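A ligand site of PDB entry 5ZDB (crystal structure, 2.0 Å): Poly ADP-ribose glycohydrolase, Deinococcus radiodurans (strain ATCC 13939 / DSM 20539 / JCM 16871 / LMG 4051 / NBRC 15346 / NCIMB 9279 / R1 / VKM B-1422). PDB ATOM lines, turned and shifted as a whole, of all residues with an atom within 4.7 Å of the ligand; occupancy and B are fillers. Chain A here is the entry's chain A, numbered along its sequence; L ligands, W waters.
N3 of the ligand sits at hydrogen-bond distance from OD2 of Asp 85 (2.8 Å).
N of Cys 197 lies within hydrogen-bond range of O2 of the ligand, at 3.2 Å.
The backbone NH (N) of Val 199 lies within hydrogen-bond range of an oxygen (O1) of the ligand, 2.8 Å away.
An oxygen (O4) of the ligand lies within hydrogen-bond range of the backbone carbonyl oxygen (O) of Leu 231, at 2.7 Å.
The backbone NH of Gly 196 sits at hydrogen-bond distance from an oxygen (O6) of the ligand (2.9 Å).
The side-chain hydroxyl (OG1) of Thr 46 lies close to a nitrogen (N1) of the ligand (3.2 Å).
The backbone NH (N) of Gly 198 sits at hydrogen-bond distance from an oxygen (O2) of the ligand (2.8 Å).
An oxygen (O5) of the ligand lies within hydrogen-bond range of the backbone NH of Gln 82 (2.7 Å).
N of Phe 200 lies within hydrogen-bond range of O2 of the ligand, 3.1 Å away.
N of Leu 231 sits at hydrogen-bond distance from N2 of the ligand (3.3 Å).
N1 of the ligand sits at hydrogen-bond distance from N of Thr 46, at 3.0 Å.
An oxygen (O7) of the ligand sits close to the backbone NH of Gly 73 (3.5 Å).
O7 of the ligand lies within hydrogen-bond range of OE2 of Glu 83.
The backbone carbonyl oxygen (O) of Ala 194 lies close to the side-chain sulfur (SG) of Cys 197.
NE2 of Gln 82 lies within hydrogen-bond range of OG1 of Thr 46 (2.8 Å).
The backbone NH of Ser 67 lies within hydrogen-bond range of the side-chain carboxylate of Glu 83.
The side-chain sulfur (SG) of Cys 197 sits at hydrogen-bond distance from the backbone carbonyl oxygen (O) of Trp 195 (3.4 Å).
The backbone carbonyl oxygen (O) of Gly 196 is in hydrogen-bond range of the backbone NH (N) of Arg 201.
OE1 of Gln 82 is in hydrogen-bond range of N of Phe 65, at 2.8 Å.
The backbone NH (N) of Gly 72 lies within hydrogen-bond range of the side-chain carboxylate (OE1) of Glu 83 (3.1 Å).
The side-chain carboxylate (OE2) of Glu 83 sits at hydrogen-bond distance from the backbone NH (N) of Gly 73, 3.4 Å away.
Thr 45 touches the ligand (CA to N1, 3.5 Å).
O of Phe 65 touches C15 of the ligand, at 3.4 Å.
C of Ala 66 touches C11 of the ligand (3.9 Å).
CB of Ser 67 touches O7 of the ligand, at 3.4 Å.
C of Gly 72 touches O7 of the ligand, 3.8 Å away.
Gln 80 touches the ligand.
Ala 81 touches the ligand.
Ala 194 touches the ligand (O to C14, 3.2 Å).
Ala 229 touches the ligand.
Within 4 Å of the ligand: Thr 45, Thr 46, Phe 65, Ala 66, Ser 67, Gly 72, Gly 73, Gln 80, Ala 81, Gln 82, Glu 83, Asp 85, Ala 194, Gly 196, Cys 197, Gly 198, Val 199, Phe 200, Ala 229 and Leu 231.
Water W3 lies within hydrogen-bond range of an oxygen (O8) of the ligand (2.5 Å), the backbone carbonyl oxygen (O) of Cys 197 (2.7 Å) and the side-chain hydroxyl (OG1) of Thr 239 (3.0 Å).
Water W5 lies within hydrogen-bond range of O5 of the ligand (2.6 Å), O of Phe 65 (2.7 Å), N of Glu 83 (2.9 Å) and N of Gln 82 (3.3 Å).
Water W7 lies within hydrogen-bond range of an oxygen (O1) of the ligand and the backbone carbonyl oxygen of Gln 80.
Water W2 lies within hydrogen-bond range of O6 of the ligand (2.8 Å), N of Ala 150 (3.0 Å), O of Ala 66 (3.0 Å) and NE1 of Trp 195 (3.3 Å).
Water W4 lies within hydrogen-bond range of an oxygen (O10) of the ligand and the side-chain hydroxyl (OG) of Ser 67.
Water W1 lies within hydrogen-bond range of O of Ala 229 (2.7 Å), N of Ala 194 (2.9 Å) and N2 of the ligand (3.0 Å).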
ATOM      1  N   GLU A  44       3.435 -25.031 -10.495  1.00  0.00           N
ATOM      2  CA  GLU A  44       3.930 -25.547 -11.775  1.00  0.00           C
ATOM      3  C   GLU A  44       4.164 -24.432 -12.796  1.00  0.00           C
ATOM      4  O   GLU A  44       3.546 -23.360 -12.756  1.00  0.00           O
ATOM      5  CB  GLU A  44       2.920 -26.543 -12.371  1.00  0.00           C
ATOM      6  CG  GLU A  44       2.478 -27.656 -11.422  1.00  0.00           C
ATOM      7  CD  GLU A  44       1.288 -28.425 -11.973  1.00  0.00           C
ATOM      8  OE1 GLU A  44       1.500 -29.534 -12.528  1.00  0.00           O
ATOM      9  OE2 GLU A  44       0.145 -27.917 -11.852  1.00  0.00           O
ATOM     10  N   THR A  45       5.045 -24.706 -13.756  1.00  0.00           N
ATOM     11  CA  THR A  45       5.055 -23.923 -14.989  1.00  0.00           C
ATOM     12  C   THR A  45       3.761 -24.149 -15.779  1.00  0.00           C
ATOM     13  O   THR A  45       3.011 -25.105 -15.566  1.00  0.00           O
ATOM     14  CB  THR A  45       6.231 -24.276 -15.894  1.00  0.00           C
ATOM     15  OG1 THR A  45       6.104 -25.647 -16.302  1.00  0.00           O
ATOM     16  CG2 THR A  45       7.548 -24.060 -15.198  1.00  0.00           C
ATOM     17  N   THR A  46       3.535 -23.258 -16.739  1.00  0.00           N
ATOM     18  CA  THR A  46       2.372 -23.405 -17.621  1.00  0.00           C
ATOM     19  C   THR A  46       2.371 -24.757 -18.320  1.00  0.00           C
ATOM     20  O   THR A  46       1.361 -25.480 -18.294  1.00  0.00           O
ATOM     21  CB  THR A  46       2.371 -22.267 -18.641  1.00  0.00           C
ATOM     22  OG1 THR A  46       2.371 -21.008 -17.952  1.00  0.00           O
ATOM     23  CG2 THR A  46       1.118 -22.361 -19.560  1.00  0.00           C
ATOM     24  N   PHE A  65       1.347 -15.550 -21.796  1.00  0.00           N
ATOM     25  CA  PHE A  65       1.467 -14.189 -21.241  1.00  0.00           C
ATOM     26  C   PHE A  65       2.261 -13.360 -22.248  1.00  0.00           C
ATOM     27  O   PHE A  65       3.441 -13.072 -22.080  1.00  0.00           O
ATOM     28  CB  PHE A  65       2.169 -14.161 -19.887  1.00  0.00           C
ATOM     29  CG  PHE A  65       1.604 -15.084 -18.843  1.00  0.00           C
ATOM     30  CD1 PHE A  65       2.357 -15.405 -17.720  1.00  0.00           C
ATOM     31  CD2 PHE A  65       0.321 -15.626 -18.965  1.00  0.00           C
ATOM     32  CE1 PHE A  65       1.860 -16.248 -16.731  1.00  0.00           C
ATOM     33  CE2 PHE A  65      -0.192 -16.483 -17.980  1.00  0.00           C
ATOM     34  CZ  PHE A  65       0.573 -16.787 -16.869  1.00  0.00           C
ATOM     35  N   ALA A  66       1.564 -12.947 -23.305  1.00  0.00           N
ATOM     36  CA  ALA A  66       2.212 -12.591 -24.555  1.00  0.00           C
ATOM     37  C   ALA A  66       2.693 -11.156 -24.596  1.00  0.00           C
ATOM     38  O   ALA A  66       2.137 -10.264 -23.940  1.00  0.00           O
ATOM     39  CB  ALA A  66       1.248 -12.828 -25.714  1.00  0.00           C
ATOM     40  N   SER A  67       3.744 -10.943 -25.405  1.00  0.00           N
ATOM     41  CA  SER A  67       4.027  -9.608 -25.900  1.00  0.00           C
ATOM     42  C   SER A  67       2.901  -9.148 -26.819  1.00  0.00           C
ATOM     43  O   SER A  67       2.277  -9.947 -27.521  1.00  0.00           O
ATOM     44  CB  SER A  67       5.360  -9.586 -26.650  1.00  0.00           C
ATOM     45  OG  SER A  67       5.532  -8.387 -27.386  1.00  0.00           O
ATOM     46  N   GLY A  72       6.900 -13.883 -29.203  1.00  0.00           N
ATOM     47  CA  GLY A  72       7.888 -14.300 -28.235  1.00  0.00           C
ATOM     48  C   GLY A  72       8.582 -13.162 -27.512  1.00  0.00           C
ATOM     49  O   GLY A  72       9.554 -13.368 -26.776  1.00  0.00           O
ATOM     50  N   GLY A  73       8.079 -11.943 -27.700  1.00  0.00           N
ATOM     51  CA  GLY A  73       8.670 -10.781 -27.071  1.00  0.00           C
ATOM     52  C   GLY A  73      10.092 -10.502 -27.509  1.00  0.00           C
ATOM     53  O   GLY A  73      10.820  -9.816 -26.785  1.00  0.00           O
ATOM     54  N   LEU A  76      13.911 -10.812 -25.290  1.00  0.00           N
ATOM     55  CA  LEU A  76      14.706  -9.771 -24.652  1.00  0.00           C
ATOM     56  C   LEU A  76      14.227  -9.519 -23.228  1.00  0.00           C
ATOM     57  O   LEU A  76      13.013  -9.576 -22.948  1.00  0.00           O
ATOM     58  CB  LEU A  76      14.647  -8.450 -25.438  1.00  0.00           C
ATOM     59  CG  LEU A  76      14.755  -8.469 -26.954  1.00  0.00           C
ATOM     60  CD1 LEU A  76      13.971  -7.308 -27.539  1.00  0.00           C
ATOM     61  CD2 LEU A  76      16.204  -8.407 -27.407  1.00  0.00           C
ATOM     62  N   GLN A  80      13.494 -15.688 -17.963  1.00  0.00           N
ATOM     63  CA  GLN A  80      12.536 -15.803 -16.872  1.00  0.00           C
ATOM     64  C   GLN A  80      11.096 -15.337 -17.274  1.00  0.00           C
ATOM     65  O   GLN A  80      10.146 -15.217 -16.461  1.00  0.00           O
ATOM     66  CB  GLN A  80      13.064 -15.027 -15.662  1.00  0.00           C
ATOM     67  CG  GLN A  80      12.375 -13.686 -15.346  1.00  0.00           C
ATOM     68  CD  GLN A  80      12.767 -12.565 -16.290  1.00  0.00           C
ATOM     69  OE1 GLN A  80      13.551 -12.755 -17.219  1.00  0.00           O
ATOM     70  NE2 GLN A  80      12.207 -11.374 -16.057  1.00  0.00           N
ATOM     71  N   ALA A  81      10.953 -15.128 -18.588  1.00  0.00           N
ATOM     72  CA  ALA A  81       9.704 -14.721 -19.199  1.00  0.00           C
ATOM     73  C   ALA A  81       8.917 -15.943 -19.658  1.00  0.00           C
ATOM     74  O   ALA A  81       9.459 -16.826 -20.339  1.00  0.00           O
ATOM     75  CB  ALA A  81       9.970 -13.786 -20.372  1.00  0.00           C
ATOM     76  N   GLN A  82       7.635 -15.976 -19.292  1.00  0.00           N
ATOM     77  CA  GLN A  82       6.810 -17.150 -19.572  1.00  0.00           C
ATOM     78  C   GLN A  82       6.679 -17.407 -21.077  1.00  0.00           C
ATOM     79  O   GLN A  82       6.796 -18.552 -21.524  1.00  0.00           O
ATOM     80  CB  GLN A  82       5.430 -16.964 -18.936  1.00  0.00           C
ATOM     81  CG  GLN A  82       4.509 -18.195 -18.990  1.00  0.00           C
ATOM     82  CD  GLN A  82       3.373 -18.037 -19.960  1.00  0.00           C
ATOM     83  OE1 GLN A  82       3.437 -17.223 -20.880  1.00  0.00           O
ATOM     84  NE2 GLN A  82       2.312 -18.824 -19.777  1.00  0.00           N
ATOM     85  N   GLU A  83       6.423 -16.364 -21.872  1.00  0.00           N
ATOM     86  CA  GLU A  83       6.263 -16.591 -23.308  1.00  0.00           C
ATOM     87  C   GLU A  83       7.539 -17.185 -23.918  1.00  0.00           C
ATOM     88  O   GLU A  83       7.473 -18.019 -24.823  1.00  0.00           O
ATOM     89  CB  GLU A  83       5.883 -15.299 -24.046  1.00  0.00           C
ATOM     90  CG  GLU A  83       5.694 -15.509 -25.579  1.00  0.00           C
ATOM     91  CD  GLU A  83       5.140 -14.287 -26.315  1.00  0.00           C
ATOM     92  OE1 GLU A  83       4.440 -14.453 -27.327  1.00  0.00           O
ATOM     93  OE2 GLU A  83       5.413 -13.144 -25.875  1.00  0.00           O
ATOM     94  N   ASP A  85       9.706 -19.159 -22.338  1.00  0.00           N
ATOM     95  CA  ASP A  85       9.613 -20.575 -21.982  1.00  0.00           C
ATOM     96  C   ASP A  85       8.721 -21.319 -22.960  1.00  0.00           C
ATOM     97  O   ASP A  85       9.112 -22.361 -23.502  1.00  0.00           O
ATOM     98  CB  ASP A  85       9.075 -20.737 -20.554  1.00  0.00           C
ATOM     99  CG  ASP A  85      10.017 -20.153 -19.503  1.00  0.00           C
ATOM    100  OD1 ASP A  85      11.177 -19.848 -19.833  1.00  0.00           O
ATOM    101  OD2 ASP A  85       9.579 -19.996 -18.335  1.00  0.00           O
ATOM    102  N   ALA A 150      -1.424  -8.855 -21.491  1.00  0.00           N
ATOM    103  CA  ALA A 150      -1.969  -8.046 -20.426  1.00  0.00           C
ATOM    104  C   ALA A 150      -1.573  -6.594 -20.695  1.00  0.00           C
ATOM    105  O   ALA A 150      -0.577  -6.348 -21.378  1.00  0.00           O
ATOM    106  CB  ALA A 150      -1.439  -8.517 -19.060  1.00  0.00           C
ATOM    107  N   ALA A 194      -0.283 -16.023 -13.517  1.00  0.00           N
ATOM    108  CA  ALA A 194       0.008 -14.637 -13.131  1.00  0.00           C
ATOM    109  C   ALA A 194       0.236 -13.729 -14.352  1.00  0.00           C
ATOM    110  O   ALA A 194       1.233 -13.025 -14.489  1.00  0.00           O
ATOM    111  CB  ALA A 194       1.213 -14.603 -12.190  1.00  0.00           C
ATOM    112  N   TRP A 195      -0.768 -13.735 -15.226  1.00  0.00           N
ATOM    113  CA  TRP A 195      -0.757 -12.918 -16.436  1.00  0.00           C
ATOM    114  C   TRP A 195      -0.459 -11.453 -16.117  1.00  0.00           C
ATOM    115  O   TRP A 195      -1.096 -10.851 -15.238  1.00  0.00           O
ATOM    116  CB  TRP A 195      -2.123 -13.084 -17.108  1.00  0.00           C
ATOM    117  CG  TRP A 195      -2.274 -12.519 -18.441  1.00  0.00           C
ATOM    118  CD1 TRP A 195      -1.365 -12.557 -19.472  1.00  0.00           C
ATOM    119  CD2 TRP A 195      -3.437 -11.851 -18.940  1.00  0.00           C
ATOM    120  NE1 TRP A 195      -1.911 -11.932 -20.604  1.00  0.00           N
ATOM    121  CE2 TRP A 195      -3.172 -11.484 -20.281  1.00  0.00           C
ATOM    122  CE3 TRP A 195      -4.673 -11.517 -18.369  1.00  0.00           C
ATOM    123  CZ2 TRP A 195      -4.105 -10.809 -21.067  1.00  0.00           C
ATOM    124  CZ3 TRP A 195      -5.597 -10.839 -19.152  1.00  0.00           C
ATOM    125  CH2 TRP A 195      -5.303 -10.492 -20.493  1.00  0.00           C
ATOM    126  N   GLY A 196       0.530 -10.878 -16.806  1.00  0.00           N
ATOM    127  CA  GLY A 196       0.887  -9.490 -16.616  1.00  0.00           C
ATOM    128  C   GLY A 196       1.609  -9.136 -15.327  1.00  0.00           C
ATOM    129  O   GLY A 196       1.898  -7.949 -15.104  1.00  0.00           O
ATOM    130  N   CYS A 197       1.917 -10.102 -14.472  1.00  0.00           N
ATOM    131  CA  CYS A 197       2.423  -9.838 -13.122  1.00  0.00           C
ATOM    132  C   CYS A 197       3.951  -9.850 -13.019  1.00  0.00           C
ATOM    133  O   CYS A 197       4.487  -9.698 -11.911  1.00  0.00           O
ATOM    134  CB  CYS A 197       1.853 -10.871 -12.145  1.00  0.00           C
ATOM    135  SG  CYS A 197       0.055 -10.834 -12.070  1.00  0.00           S
ATOM    136  N   GLY A 198       4.661 -10.027 -14.119  1.00  0.00           N
ATOM    137  CA  GLY A 198       6.117 -10.033 -14.037  1.00  0.00           C
ATOM    138  C   GLY A 198       6.681  -8.862 -14.792  1.00  0.00           C
ATOM    139  O   GLY A 198       6.776  -7.732 -14.277  1.00  0.00           O
ATOM    140  N   VAL A 199       7.040  -9.105 -16.055  1.00  0.00           N
ATOM    141  CA  VAL A 199       7.574  -8.061 -16.910  1.00  0.00           C
ATOM    142  C   VAL A 199       6.621  -6.876 -17.013  1.00  0.00           C
ATOM    143  O   VAL A 199       7.054  -5.717 -17.040  1.00  0.00           O
ATOM    144  CB  VAL A 199       7.902  -8.679 -18.280  1.00  0.00           C
ATOM    145  CG1 VAL A 199       8.278  -7.592 -19.293  1.00  0.00           C
ATOM    146  CG2 VAL A 199       9.050  -9.721 -18.100  1.00  0.00           C
ATOM    147  N   PHE A 200       5.301  -7.134 -17.066  1.00  0.00           N
ATOM    148  CA  PHE A 200       4.329  -6.049 -17.261  1.00  0.00           C
ATOM    149  C   PHE A 200       3.873  -5.405 -15.951  1.00  0.00           C
ATOM    150  O   PHE A 200       3.043  -4.490 -15.992  1.00  0.00           O
ATOM    151  CB  PHE A 200       3.094  -6.537 -18.029  1.00  0.00           C
ATOM    152  CG  PHE A 200       3.329  -6.667 -19.523  1.00  0.00           C
ATOM    153  CD1 PHE A 200       4.552  -6.342 -20.082  1.00  0.00           C
ATOM    154  CD2 PHE A 200       2.324  -7.176 -20.334  1.00  0.00           C
ATOM    155  CE1 PHE A 200       4.775  -6.469 -21.449  1.00  0.00           C
ATOM    156  CE2 PHE A 200       2.530  -7.317 -21.705  1.00  0.00           C
ATOM    157  CZ  PHE A 200       3.768  -6.960 -22.269  1.00  0.00           C
ATOM    158  N   ARG A 201       4.349  -5.905 -14.802  1.00  0.00           N
ATOM    159  CA  ARG A 201       4.302  -5.173 -13.526  1.00  0.00           C
ATOM    160  C   ARG A 201       2.889  -4.926 -13.034  1.00  0.00           C
ATOM    161  O   ARG A 201       2.620  -3.929 -12.354  1.00  0.00           O
ATOM    162  CB  ARG A 201       5.056  -3.841 -13.624  1.00  0.00           C
ATOM    163  CG  ARG A 201       6.512  -4.004 -14.041  1.00  0.00           C
ATOM    164  CD  ARG A 201       7.330  -4.670 -12.955  1.00  0.00           C
ATOM    165  NE  ARG A 201       8.543  -3.931 -12.637  1.00  0.00           N
ATOM    166  CZ  ARG A 201       9.139  -3.938 -11.453  1.00  0.00           C
ATOM    167  NH1 ARG A 201       8.623  -4.656 -10.454  1.00  0.00           N
ATOM    168  NH2 ARG A 201      10.242  -3.229 -11.247  1.00  0.00           N
ATOM    169  N   ALA A 229      -1.398 -22.106 -12.714  1.00  0.00           N
ATOM    170  CA  ALA A 229      -0.014 -22.565 -12.569  1.00  0.00           C
ATOM    171  C   ALA A 229       0.876 -21.338 -12.470  1.00  0.00           C
ATOM    172  O   ALA A 229       1.031 -20.596 -13.442  1.00  0.00           O
ATOM    173  CB  ALA A 229       0.399 -23.467 -13.734  1.00  0.00           C
ATOM    174  N   VAL A 230       1.466 -21.128 -11.295  1.00  0.00           N
ATOM    175  CA  VAL A 230       2.203 -19.910 -10.999  1.00  0.00           C
ATOM    176  C   VAL A 230       3.637 -20.314 -10.699  1.00  0.00           C
ATOM    177  O   VAL A 230       3.933 -20.865  -9.621  1.00  0.00           O
ATOM    178  CB  VAL A 230       1.587 -19.111  -9.846  1.00  0.00           C
ATOM    179  CG1 VAL A 230       2.398 -17.825  -9.585  1.00  0.00           C
ATOM    180  CG2 VAL A 230       0.124 -18.790 -10.152  1.00  0.00           C
ATOM    181  N   LEU A 231       4.529 -20.090 -11.642  1.00  0.00           N
ATOM    182  CA  LEU A 231       5.935 -20.279 -11.351  1.00  0.00           C
ATOM    183  C   LEU A 231       6.413 -19.127 -10.488  1.00  0.00           C
ATOM    184  O   LEU A 231       6.143 -17.967 -10.799  1.00  0.00           O
ATOM    185  CB  LEU A 231       6.756 -20.357 -12.638  1.00  0.00           C
ATOM    186  CG  LEU A 231       8.263 -20.470 -12.394  1.00  0.00           C
ATOM    187  CD1 LEU A 231       8.561 -21.812 -11.769  1.00  0.00           C
ATOM    188  CD2 LEU A 231       8.989 -20.297 -13.718  1.00  0.00           C
ATOM    189  N   THR A 239       4.169 -13.996  -5.471  1.00  0.00           N
ATOM    190  CA  THR A 239       3.188 -14.092  -6.540  1.00  0.00           C
ATOM    191  C   THR A 239       2.291 -15.316  -6.373  1.00  0.00           C
ATOM    192  O   THR A 239       1.064 -15.210  -6.451  1.00  0.00           O
ATOM    193  CB  THR A 239       3.886 -14.106  -7.901  1.00  0.00           C
ATOM    194  OG1 THR A 239       4.694 -12.930  -8.013  1.00  0.00           O
ATOM    195  CG2 THR A 239       2.850 -14.140  -9.039  1.00  0.00           C
HETATM  196  N1  LIG L   1       5.123 -20.726 -16.317  1.00  0.00           N
HETATM  197  C1  LIG L   1       4.203 -20.265 -15.421  1.00  0.00           C
HETATM  198  N2  LIG L   1       4.388 -19.074 -14.794  1.00  0.00           N
HETATM  199  C2  LIG L   1       5.494 -18.354 -15.082  1.00  0.00           C
HETATM  200  C3  LIG L   1       6.395 -18.803 -15.970  1.00  0.00           C
HETATM  201  C4  LIG L   1       6.207 -20.009 -16.606  1.00  0.00           C
HETATM  202  N3  LIG L   1       6.960 -20.769 -17.584  1.00  0.00           N
HETATM  203  N4  LIG L   1       7.394 -17.911 -16.062  1.00  0.00           N
HETATM  204  C5  LIG L   1       7.108 -16.908 -15.247  1.00  0.00           C
HETATM  205  N5  LIG L   1       5.943 -17.168 -14.632  1.00  0.00           N
HETATM  206  P1  LIG L   1       5.760 -12.844 -17.353  1.00  0.00           P
HETATM  207  P2  LIG L   1       3.977 -10.659 -18.185  1.00  0.00           P
HETATM  208  C6  LIG L   1       5.329 -16.357 -13.644  1.00  0.00           C
HETATM  209  O1  LIG L   1       6.577 -11.741 -16.729  1.00  0.00           O
HETATM  210  O2  LIG L   1       4.068  -9.917 -16.869  1.00  0.00           O
HETATM  211  C7  LIG L   1       7.620 -11.518 -21.997  1.00  0.00           C
HETATM  212  O3  LIG L   1       8.722 -11.011 -22.359  1.00  0.00           O
HETATM  213  C8  LIG L   1       6.186 -15.554 -12.956  1.00  0.00           C
HETATM  214  O4  LIG L   1       5.720 -15.364 -11.572  1.00  0.00           O
HETATM  215  O5  LIG L   1       6.458 -13.655 -18.428  1.00  0.00           O
HETATM  216  O6  LIG L   1       2.625 -10.670 -18.815  1.00  0.00           O
HETATM  217  C9  LIG L   1       6.547 -11.329 -23.079  1.00  0.00           C
HETATM  218  O7  LIG L   1       7.145 -11.479 -24.403  1.00  0.00           O
HETATM  219  C10 LIG L   1       6.046 -14.175 -13.629  1.00  0.00           C
HETATM  220  O8  LIG L   1       6.316 -13.207 -12.760  1.00  0.00           O
HETATM  221  O9  LIG L   1       4.381 -12.239 -18.037  1.00  0.00           O
HETATM  222  C11 LIG L   1       6.051 -10.096 -22.888  1.00  0.00           C
HETATM  223  O10 LIG L   1       6.806  -9.044 -23.532  1.00  0.00           O
HETATM  224  C12 LIG L   1       4.501 -14.150 -13.981  1.00  0.00           C
HETATM  225  O11 LIG L   1       4.233 -15.389 -14.341  1.00  0.00           O
HETATM  226  C13 LIG L   1       6.132  -9.912 -21.271  1.00  0.00           C
HETATM  227  O12 LIG L   1       7.086 -10.661 -20.785  1.00  0.00           O
HETATM  228  C14 LIG L   1       4.351 -13.284 -15.218  1.00  0.00           C
HETATM  229  O13 LIG L   1       5.216 -13.838 -16.181  1.00  0.00           O
HETATM  230  C15 LIG L   1       4.808 -10.312 -20.640  1.00  0.00           C
HETATM  231  O14 LIG L   1       4.977  -9.939 -19.297  1.00  0.00           O
HETATM  232  O   HOH W   1       1.887 -18.017 -13.624  1.00  0.00           O
HETATM  233  O   HOH W   2       1.044 -10.449 -21.114  1.00  0.00           O
HETATM  234  O   HOH W   3       5.266 -12.022 -10.780  1.00  0.00           O
HETATM  235  O   HOH W   4       6.970  -6.560 -25.095  1.00  0.00           O
HETATM  236  O   HOH W   5       5.854 -13.702 -20.922  1.00  0.00           O
HETATM  237  O   HOH W   6       6.078 -23.341 -19.166  1.00  0.00           O
HETATM  238  O   HOH W   7       9.024 -12.404 -15.648  1.00  0.00           O
